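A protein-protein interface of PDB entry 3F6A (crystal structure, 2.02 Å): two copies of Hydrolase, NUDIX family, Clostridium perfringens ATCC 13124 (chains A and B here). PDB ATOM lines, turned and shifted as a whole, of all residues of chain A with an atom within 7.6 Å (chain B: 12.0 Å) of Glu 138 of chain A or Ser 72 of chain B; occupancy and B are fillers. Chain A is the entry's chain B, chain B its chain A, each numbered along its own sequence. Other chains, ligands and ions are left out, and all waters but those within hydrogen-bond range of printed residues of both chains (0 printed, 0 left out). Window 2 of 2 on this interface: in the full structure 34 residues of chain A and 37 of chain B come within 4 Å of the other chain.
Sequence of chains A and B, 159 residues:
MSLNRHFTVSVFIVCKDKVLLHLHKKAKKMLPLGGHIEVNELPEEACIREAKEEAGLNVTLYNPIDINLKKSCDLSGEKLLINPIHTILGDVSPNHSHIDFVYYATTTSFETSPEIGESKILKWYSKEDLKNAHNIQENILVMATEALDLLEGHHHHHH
The side-chain amide oxygen (OD1) of Asn 139 of chain A is in hydrogen-bond range of the side-chain hydroxyl (OG) of Ser 76 of chain B (2.9 Å). The side-chain carboxylate (OE1) of Glu 78 of chain B lies within hydrogen-bond range of the side-chain amide nitrogen (ND2) of Asn 139 of chain A.
O of Asn 68 of chain B sits at hydrogen-bond distance from OG of Ser 72 of chain B. The backbone carbonyl oxygen (O) of Leu 69 of chain B sits at hydrogen-bond distance from the side-chain hydroxyl (OG) of Ser 72 of chain B (3.1 Å). The backbone carbonyl oxygen (O) of Leu 69 of chain B sits close to the side-chain sulfur (SG) of Cys 73 of chain B, 3.2 Å away. The backbone carbonyl oxygen of Ser 72 of chain B lies within hydrogen-bond range of the side-chain hydroxyl of Ser 76 of chain B (2.9 Å). O of Cys 73 of chain B sits at hydrogen-bond distance from N of Glu 78 of chain B (2.8 Å). The side-chain hydroxyl (OG1) of Thr 145 of chain A is in hydrogen-bond range of the backbone carbonyl oxygen (O) of Val 142 of chain A, at 2.4 Å.
Among the printed residues, pairs that only touch across the chains: Glu 138 of chain A with Ser 72 of chain B, Asn 139 of chain A with Leu 69 of chain B, Asn 139 of chain A with Ser 72 of chain B, Asn 139 of chain A with Cys 73 of chain B, Val 142 of chain A with Asn 68 of chain B, Val 142 of chain A with Leu 69 of chain B, Val 142 of chain A with Ser 72 of chain B and Met 143 of chain A with Leu 69 of chain B.
No residue of chain B comes within 4 Å of Gln 137 of chain A. Glu 138 of chain A touches just one residue of chain B: Ser 72 (3.7 Å). Asn 139 of chain A touches five residues of chain B. Of the printed residues of chain B, Met 143 of chain A touches Leu 69 (3.5 Å). Ser 72 of chain B touches just these residues of chain A: Glu 138, Asn 139 and Val 142. Of the printed residues of chain A, Ser 76 of chain B touches Asn 139. Gly 77 of chain B touches none of the printed residues of chain A. Lys 79 of chain B touches none of the printed residues of chain A. The nearest residue of chain B that does not touch Glu 138 of chain A is Ser 76 of chain B (4.4 Å). The nearest residue of chain A that does not touch Ser 72 of chain B is Ile 140 of chain A (5.8 Å). The nearest printed residue of chain A that does not touch Leu 69 of chain B is Ile 140 of chain A (5.7 Å).
Of the 11 printed residues of chain A, 4 touch a printed residue of chain B. Hydrophobic or aromatic side chains of chain A within 4 Å of the printed part of chain B: Val 142 and Met 143. Of the 17 printed residues of chain B, 6 touch a printed residue of chain A. Hydrophobic or aromatic side chains of chain B within 4 Å of the printed part of chain A: Leu 69. Along chain B the printed residues that touch a printed residue of chain A span positions 68 to 78. Among the printed residues, no Asp or Glu carboxylate lies within 4 Å of a Lys or Arg side-chain nitrogen of the other chain.
No position is printed for both chains.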
ATOM      1  N   ASN A 135      11.556 -19.997  39.148  1.00  0.00           N
ATOM      2  CA  ASN A 135      10.668 -20.982  38.544  1.00  0.00           C
ATOM      3  C   ASN A 135      10.899 -21.267  37.063  1.00  0.00           C
ATOM      4  O   ASN A 135       9.951 -21.476  36.309  1.00  0.00           O
ATOM      5  CB  ASN A 135       9.219 -20.547  38.764  1.00  0.00           C
ATOM      6  CG  ASN A 135       8.972 -19.120  38.316  1.00  0.00           C
ATOM      7  OD1 ASN A 135       9.878 -18.448  37.814  1.00  0.00           O
ATOM      8  ND2 ASN A 135       7.749 -18.646  38.497  1.00  0.00           N
ATOM      9  N   ILE A 136      12.159 -21.291  36.643  1.00  0.00           N
ATOM     10  CA  ILE A 136      12.472 -21.573  35.248  1.00  0.00           C
ATOM     11  C   ILE A 136      13.440 -22.752  35.158  1.00  0.00           C
ATOM     12  O   ILE A 136      14.533 -22.698  35.720  1.00  0.00           O
ATOM     13  CB  ILE A 136      13.130 -20.362  34.565  1.00  0.00           C
ATOM     14  CG1 ILE A 136      12.196 -19.155  34.619  1.00  0.00           C
ATOM     15  CG2 ILE A 136      13.482 -20.716  33.127  1.00  0.00           C
ATOM     16  CD1 ILE A 136      12.745 -17.913  33.924  1.00  0.00           C
ATOM     17  N   GLN A 137      13.036 -23.806  34.452  1.00  0.00           N
ATOM     18  CA  GLN A 137      13.874 -24.988  34.291  1.00  0.00           C
ATOM     19  C   GLN A 137      15.115 -24.661  33.467  1.00  0.00           C
ATOM     20  O   GLN A 137      15.093 -23.787  32.603  1.00  0.00           O
ATOM     21  CB  GLN A 137      13.078 -26.109  33.631  1.00  0.00           C
ATOM     22  CG  GLN A 137      11.993 -26.663  34.525  1.00  0.00           C
ATOM     23  CD  GLN A 137      10.990 -27.500  33.765  1.00  0.00           C
ATOM     24  OE1 GLN A 137      10.178 -26.976  32.995  1.00  0.00           O
ATOM     25  NE2 GLN A 137      11.043 -28.813  33.968  1.00  0.00           N
ATOM     26  N   GLU A 138      16.194 -25.385  33.727  1.00  0.00           N
ATOM     27  CA  GLU A 138      17.452 -25.133  33.052  1.00  0.00           C
ATOM     28  C   GLU A 138      17.436 -25.136  31.523  1.00  0.00           C
ATOM     29  O   GLU A 138      18.051 -24.267  30.892  1.00  0.00           O
ATOM     30  CB  GLU A 138      18.514 -26.109  33.566  1.00  0.00           C
ATOM     31  CG  GLU A 138      19.916 -25.673  33.205  1.00  0.00           C
ATOM     32  CD  GLU A 138      20.253 -24.297  33.760  1.00  0.00           C
ATOM     33  OE1 GLU A 138      21.088 -23.591  33.152  1.00  0.00           O
ATOM     34  OE2 GLU A 138      19.686 -23.924  34.812  1.00  0.00           O
ATOM     35  N   ASN A 139      16.738 -26.091  30.920  1.00  0.00           N
ATOM     36  CA  ASN A 139      16.702 -26.142  29.465  1.00  0.00           C
ATOM     37  C   ASN A 139      15.979 -24.921  28.908  1.00  0.00           C
ATOM     38  O   ASN A 139      16.335 -24.425  27.836  1.00  0.00           O
ATOM     39  CB  ASN A 139      16.033 -27.431  28.985  1.00  0.00           C
ATOM     40  CG  ASN A 139      14.593 -27.531  29.413  1.00  0.00           C
ATOM     41  OD1 ASN A 139      14.259 -27.299  30.570  1.00  0.00           O
ATOM     42  ND2 ASN A 139      13.729 -27.889  28.483  1.00  0.00           N
ATOM     43  N   ILE A 140      14.977 -24.437  29.642  1.00  0.00           N
ATOM     44  CA  ILE A 140      14.212 -23.256  29.231  1.00  0.00           C
ATOM     45  C   ILE A 140      15.103 -22.020  29.356  1.00  0.00           C
ATOM     46  O   ILE A 140      15.024 -21.088  28.547  1.00  0.00           O
ATOM     47  CB  ILE A 140      12.969 -23.050  30.118  1.00  0.00           C
ATOM     48  CG1 ILE A 140      12.071 -24.289  30.061  1.00  0.00           C
ATOM     49  CG2 ILE A 140      12.210 -21.815  29.674  1.00  0.00           C
ATOM     50  CD1 ILE A 140      11.593 -24.653  28.667  1.00  0.00           C
ATOM     51  N   LEU A 141      15.937 -22.010  30.390  1.00  0.00           N
ATOM     52  CA  LEU A 141      16.864 -20.906  30.610  1.00  0.00           C
ATOM     53  C   LEU A 141      17.861 -20.839  29.454  1.00  0.00           C
ATOM     54  O   LEU A 141      18.168 -19.763  28.947  1.00  0.00           O
ATOM     55  CB  LEU A 141      17.629 -21.097  31.926  1.00  0.00           C
ATOM     56  CG  LEU A 141      16.872 -20.792  33.219  1.00  0.00           C
ATOM     57  CD1 LEU A 141      17.648 -21.306  34.437  1.00  0.00           C
ATOM     58  CD2 LEU A 141      16.658 -19.288  33.310  1.00  0.00           C
ATOM     59  N   VAL A 142      18.363 -21.993  29.034  1.00  0.00           N
ATOM     60  CA  VAL A 142      19.326 -22.028  27.937  1.00  0.00           C
ATOM     61  C   VAL A 142      18.736 -21.537  26.617  1.00  0.00           C
ATOM     62  O   VAL A 142      19.386 -20.774  25.897  1.00  0.00           O
ATOM     63  CB  VAL A 142      19.909 -23.453  27.756  1.00  0.00           C
ATOM     64  CG1 VAL A 142      20.593 -23.591  26.401  1.00  0.00           C
ATOM     65  CG2 VAL A 142      20.911 -23.725  28.867  1.00  0.00           C
ATOM     66  N   MET A 143      17.519 -21.966  26.291  1.00  0.00           N
ATOM     67  CA  MET A 143      16.892 -21.537  25.047  1.00  0.00           C
ATOM     68  C   MET A 143      16.450 -20.085  25.088  1.00  0.00           C
ATOM     69  O   MET A 143      16.522 -19.386  24.076  1.00  0.00           O
ATOM     70  CB  MET A 143      15.714 -22.441  24.703  1.00  0.00           C
ATOM     71  CG  MET A 143      16.164 -23.851  24.322  1.00  0.00           C
ATOM     72  SD  MET A 143      14.738 -24.985  23.729  1.00  0.00           S
ATOM     73  CE  MET A 143      14.014 -25.508  25.442  1.00  0.00           C
ATOM     74  N   ALA A 144      16.000 -19.623  26.251  1.00  0.00           N
ATOM     75  CA  ALA A 144      15.591 -18.229  26.382  1.00  0.00           C
ATOM     76  C   ALA A 144      16.827 -17.348  26.173  1.00  0.00           C
ATOM     77  O   ALA A 144      16.750 -16.279  25.569  1.00  0.00           O
ATOM     78  CB  ALA A 144      14.999 -17.977  27.762  1.00  0.00           C
ATOM     79  N   THR A 145      17.970 -17.806  26.673  1.00  0.00           N
ATOM     80  CA  THR A 145      19.207 -17.053  26.530  1.00  0.00           C
ATOM     81  C   THR A 145      19.680 -17.057  25.078  1.00  0.00           C
ATOM     82  O   THR A 145      20.196 -16.055  24.584  1.00  0.00           O
ATOM     83  CB  THR A 145      20.324 -17.626  27.428  1.00  0.00           C
ATOM     84  OG1 THR A 145      20.555 -18.992  27.076  1.00  0.00           O
ATOM     85  CG2 THR A 145      19.936 -17.540  28.887  1.00  0.00           C
ATOM     86  N   ILE B  65      26.116 -30.843  17.944  1.00  0.00           N
ATOM     87  CA  ILE B  65      25.505 -30.795  19.265  1.00  0.00           C
ATOM     88  C   ILE B  65      25.639 -29.436  19.940  1.00  0.00           C
ATOM     89  O   ILE B  65      26.697 -28.814  19.904  1.00  0.00           O
ATOM     90  CB  ILE B  65      26.124 -31.857  20.208  1.00  0.00           C
ATOM     91  CG1 ILE B  65      25.980 -33.258  19.607  1.00  0.00           C
ATOM     92  CG2 ILE B  65      25.449 -31.791  21.577  1.00  0.00           C
ATOM     93  CD1 ILE B  65      24.551 -33.793  19.580  1.00  0.00           C
ATOM     94  N   ASP B  66      24.538 -28.988  20.537  1.00  0.00           N
ATOM     95  CA  ASP B  66      24.471 -27.736  21.284  1.00  0.00           C
ATOM     96  C   ASP B  66      24.572 -28.295  22.704  1.00  0.00           C
ATOM     97  O   ASP B  66      23.555 -28.496  23.366  1.00  0.00           O
ATOM     98  CB  ASP B  66      23.097 -27.087  21.059  1.00  0.00           C
ATOM     99  CG  ASP B  66      22.934 -25.760  21.775  1.00  0.00           C
ATOM    100  OD1 ASP B  66      23.740 -25.439  22.675  1.00  0.00           O
ATOM    101  OD2 ASP B  66      21.972 -25.034  21.439  1.00  0.00           O
ATOM    102  N   ILE B  67      25.797 -28.574  23.147  1.00  0.00           N
ATOM    103  CA  ILE B  67      26.042 -29.181  24.459  1.00  0.00           C
ATOM    104  C   ILE B  67      25.271 -28.564  25.622  1.00  0.00           C
ATOM    105  O   ILE B  67      24.712 -29.284  26.454  1.00  0.00           O
ATOM    106  CB  ILE B  67      27.577 -29.204  24.795  1.00  0.00           C
ATOM    107  CG1 ILE B  67      27.856 -30.204  25.924  1.00  0.00           C
ATOM    108  CG2 ILE B  67      28.059 -27.822  25.218  1.00  0.00           C
ATOM    109  CD1 ILE B  67      27.572 -31.650  25.550  1.00  0.00           C
ATOM    110  N   ASN B  68      25.232 -27.238  25.684  1.00  0.00           N
ATOM    111  CA  ASN B  68      24.519 -26.547  26.753  1.00  0.00           C
ATOM    112  C   ASN B  68      23.061 -26.978  26.828  1.00  0.00           C
ATOM    113  O   ASN B  68      22.529 -27.237  27.914  1.00  0.00           O
ATOM    114  CB  ASN B  68      24.594 -25.031  26.545  1.00  0.00           C
ATOM    115  CG  ASN B  68      25.882 -24.432  27.071  1.00  0.00           C
ATOM    116  OD1 ASN B  68      26.084 -24.339  28.280  1.00  0.00           O
ATOM    117  ND2 ASN B  68      26.761 -24.026  26.167  1.00  0.00           N
ATOM    118  N   LEU B  69      22.416 -27.058  25.672  1.00  0.00           N
ATOM    119  CA  LEU B  69      21.015 -27.450  25.634  1.00  0.00           C
ATOM    120  C   LEU B  69      20.850 -28.962  25.808  1.00  0.00           C
ATOM    121  O   LEU B  69      19.874 -29.419  26.401  1.00  0.00           O
ATOM    122  CB  LEU B  69      20.383 -26.997  24.318  1.00  0.00           C
ATOM    123  CG  LEU B  69      18.868 -27.207  24.209  1.00  0.00           C
ATOM    124  CD1 LEU B  69      18.149 -26.509  25.361  1.00  0.00           C
ATOM    125  CD2 LEU B  69      18.387 -26.664  22.873  1.00  0.00           C
ATOM    126  N   LYS B  70      21.799 -29.740  25.297  1.00  0.00           N
ATOM    127  CA  LYS B  70      21.707 -31.194  25.428  1.00  0.00           C
ATOM    128  C   LYS B  70      21.734 -31.604  26.898  1.00  0.00           C
ATOM    129  O   LYS B  70      20.878 -32.355  27.352  1.00  0.00           O
ATOM    130  CB  LYS B  70      22.850 -31.886  24.681  1.00  0.00           C
ATOM    131  CG  LYS B  70      22.754 -33.411  24.706  1.00  0.00           C
ATOM    132  CD  LYS B  70      23.917 -34.072  23.994  1.00  0.00           C
ATOM    133  CE  LYS B  70      23.921 -35.580  24.236  1.00  0.00           C
ATOM    134  NZ  LYS B  70      25.111 -36.242  23.616  1.00  0.00           N
ATOM    135  N   LYS B  71      22.712 -31.095  27.642  1.00  0.00           N
ATOM    136  CA  LYS B  71      22.850 -31.421  29.059  1.00  0.00           C
ATOM    137  C   LYS B  71      21.690 -30.894  29.907  1.00  0.00           C
ATOM    138  O   LYS B  71      21.168 -31.610  30.763  1.00  0.00           O
ATOM    139  CB  LYS B  71      24.179 -30.880  29.592  1.00  0.00           C
ATOM    140  CG  LYS B  71      25.374 -31.348  28.775  1.00  0.00           C
ATOM    141  CD  LYS B  71      26.710 -30.999  29.419  1.00  0.00           C
ATOM    142  CE  LYS B  71      27.048 -31.946  30.549  1.00  0.00           C
ATOM    143  NZ  LYS B  71      28.489 -31.853  30.931  1.00  0.00           N
ATOM    144  N   SER B  72      21.281 -29.652  29.670  1.00  0.00           N
ATOM    145  CA  SER B  72      20.174 -29.091  30.430  1.00  0.00           C
ATOM    146  C   SER B  72      18.890 -29.868  30.134  1.00  0.00           C
ATOM    147  O   SER B  72      18.055 -30.054  31.019  1.00  0.00           O
ATOM    148  CB  SER B  72      19.994 -27.603  30.105  1.00  0.00           C
ATOM    149  OG  SER B  72      19.829 -27.384  28.718  1.00  0.00           O
ATOM    150  N   CYS B  73      18.738 -30.342  28.898  1.00  0.00           N
ATOM    151  CA  CYS B  73      17.551 -31.109  28.538  1.00  0.00           C
ATOM    152  C   CYS B  73      17.509 -32.421  29.317  1.00  0.00           C
ATOM    153  O   CYS B  73      16.487 -32.766  29.904  1.00  0.00           O
ATOM    154  CB  CYS B  73      17.523 -31.406  27.035  1.00  0.00           C
ATOM    155  SG  CYS B  73      16.741 -30.127  26.013  1.00  0.00           S
ATOM    156  N   ASP B  74      18.622 -33.146  29.324  1.00  0.00           N
ATOM    157  CA  ASP B  74      18.691 -34.418  30.038  1.00  0.00           C
ATOM    158  C   ASP B  74      18.288 -34.254  31.502  1.00  0.00           C
ATOM    159  O   ASP B  74      17.557 -35.082  32.046  1.00  0.00           O
ATOM    160  CB  ASP B  74      20.098 -35.015  29.949  1.00  0.00           C
ATOM    161  CG  ASP B  74      20.500 -35.347  28.524  1.00  0.00           C
ATOM    162  OD1 ASP B  74      19.646 -35.856  27.766  1.00  0.00           O
ATOM    163  OD2 ASP B  74      21.674 -35.113  28.162  1.00  0.00           O
ATOM    164  N   LEU B  75      18.770 -33.189  32.135  1.00  0.00           N
ATOM    165  CA  LEU B  75      18.437 -32.916  33.528  1.00  0.00           C
ATOM    166  C   LEU B  75      16.929 -32.758  33.667  1.00  0.00           C
ATOM    167  O   LEU B  75      16.306 -33.346  34.550  1.00  0.00           O
ATOM    168  CB  LEU B  75      19.102 -31.622  33.999  1.00  0.00           C
ATOM    169  CG  LEU B  75      20.612 -31.570  34.206  1.00  0.00           C
ATOM    170  CD1 LEU B  75      21.023 -30.136  34.515  1.00  0.00           C
ATOM    171  CD2 LEU B  75      21.009 -32.502  35.343  1.00  0.00           C
ATOM    172  N   SER B  76      16.357 -31.951  32.779  1.00  0.00           N
ATOM    173  CA  SER B  76      14.928 -31.673  32.774  1.00  0.00           C
ATOM    174  C   SER B  76      14.105 -32.888  32.353  1.00  0.00           C
ATOM    175  O   SER B  76      12.889 -32.800  32.206  1.00  0.00           O
ATOM    176  CB  SER B  76      14.640 -30.499  31.833  1.00  0.00           C
ATOM    177  OG  SER B  76      15.499 -29.397  32.103  1.00  0.00           O
ATOM    178  N   GLY B  77      14.774 -34.019  32.158  1.00  0.00           N
ATOM    179  CA  GLY B  77      14.082 -35.233  31.757  1.00  0.00           C
ATOM    180  C   GLY B  77      13.687 -35.274  30.289  1.00  0.00           C
ATOM    181  O   GLY B  77      12.862 -36.101  29.886  1.00  0.00           O
ATOM    182  N   GLU B  78      14.269 -34.386  29.484  1.00  0.00           N
ATOM    183  CA  GLU B  78      13.968 -34.333  28.055  1.00  0.00           C
ATOM    184  C   GLU B  78      15.204 -34.703  27.236  1.00  0.00           C
ATOM    185  O   GLU B  78      16.283 -34.903  27.788  1.00  0.00           O
ATOM    186  CB  GLU B  78      13.497 -32.927  27.666  1.00  0.00           C
ATOM    187  CG  GLU B  78      12.226 -32.482  28.372  1.00  0.00           C
ATOM    188  CD  GLU B  78      11.835 -31.063  28.017  1.00  0.00           C
ATOM    189  OE1 GLU B  78      12.651 -30.149  28.249  1.00  0.00           O
ATOM    190  OE2 GLU B  78      10.713 -30.854  27.510  1.00  0.00           O
ATOM    191  N   LYS B  79      15.051 -34.795  25.919  1.00  0.00           N
ATOM    192  CA  LYS B  79      16.184 -35.135  25.070  1.00  0.00           C
ATOM    193  C   LYS B  79      16.259 -34.283  23.814  1.00  0.00           C
ATOM    194  O   LYS B  79      15.298 -34.187  23.051  1.00  0.00           O
ATOM    195  CB  LYS B  79      16.144 -36.620  24.694  1.00  0.00           C
ATOM    196  CG  LYS B  79      16.391 -37.550  25.876  1.00  0.00           C
ATOM    197  CD  LYS B  79      16.496 -39.011  25.457  1.00  0.00           C
ATOM    198  CE  LYS B  79      16.779 -39.903  26.666  1.00  0.00           C
ATOM    199  NZ  LYS B  79      16.897 -41.346  26.304  1.00  0.00           N
ATOM    200  N   LEU B  80      17.413 -33.658  23.620  1.00  0.00           N
ATOM    201  CA  LEU B  80      17.656 -32.819  22.458  1.00  0.00           C
ATOM    202  C   LEU B  80      17.932 -33.745  21.279  1.00  0.00           C
ATOM    203  O   LEU B  80      18.890 -34.525  21.295  1.00  0.00           O
ATOM    204  CB  LEU B  80      18.862 -31.909  22.705  1.00  0.00           C
ATOM    205  CG  LEU B  80      19.221 -30.956  21.564  1.00  0.00           C
ATOM    206  CD1 LEU B  80      18.128 -29.905  21.406  1.00  0.00           C
ATOM    207  CD2 LEU B  80      20.559 -30.296  21.855  1.00  0.00           C
ATOM    208  N   LEU B  81      17.086 -33.659  20.261  1.00  0.00           N
ATOM    209  CA  LEU B  81      17.220 -34.509  19.089  1.00  0.00           C
ATOM    210  C   LEU B  81      18.028 -33.838  17.990  1.00  0.00           C
ATOM    211  O   LEU B  81      18.319 -32.647  18.064  1.00  0.00           O
ATOM    212  CB  LEU B  81      15.831 -34.859  18.550  1.00  0.00           C
ATOM    213  CG  LEU B  81      14.845 -35.446  19.556  1.00  0.00           C
ATOM    214  CD1 LEU B  81      13.490 -35.631  18.883  1.00  0.00           C
ATOM    215  CD2 LEU B  81      15.374 -36.767  20.095  1.00  0.00           C
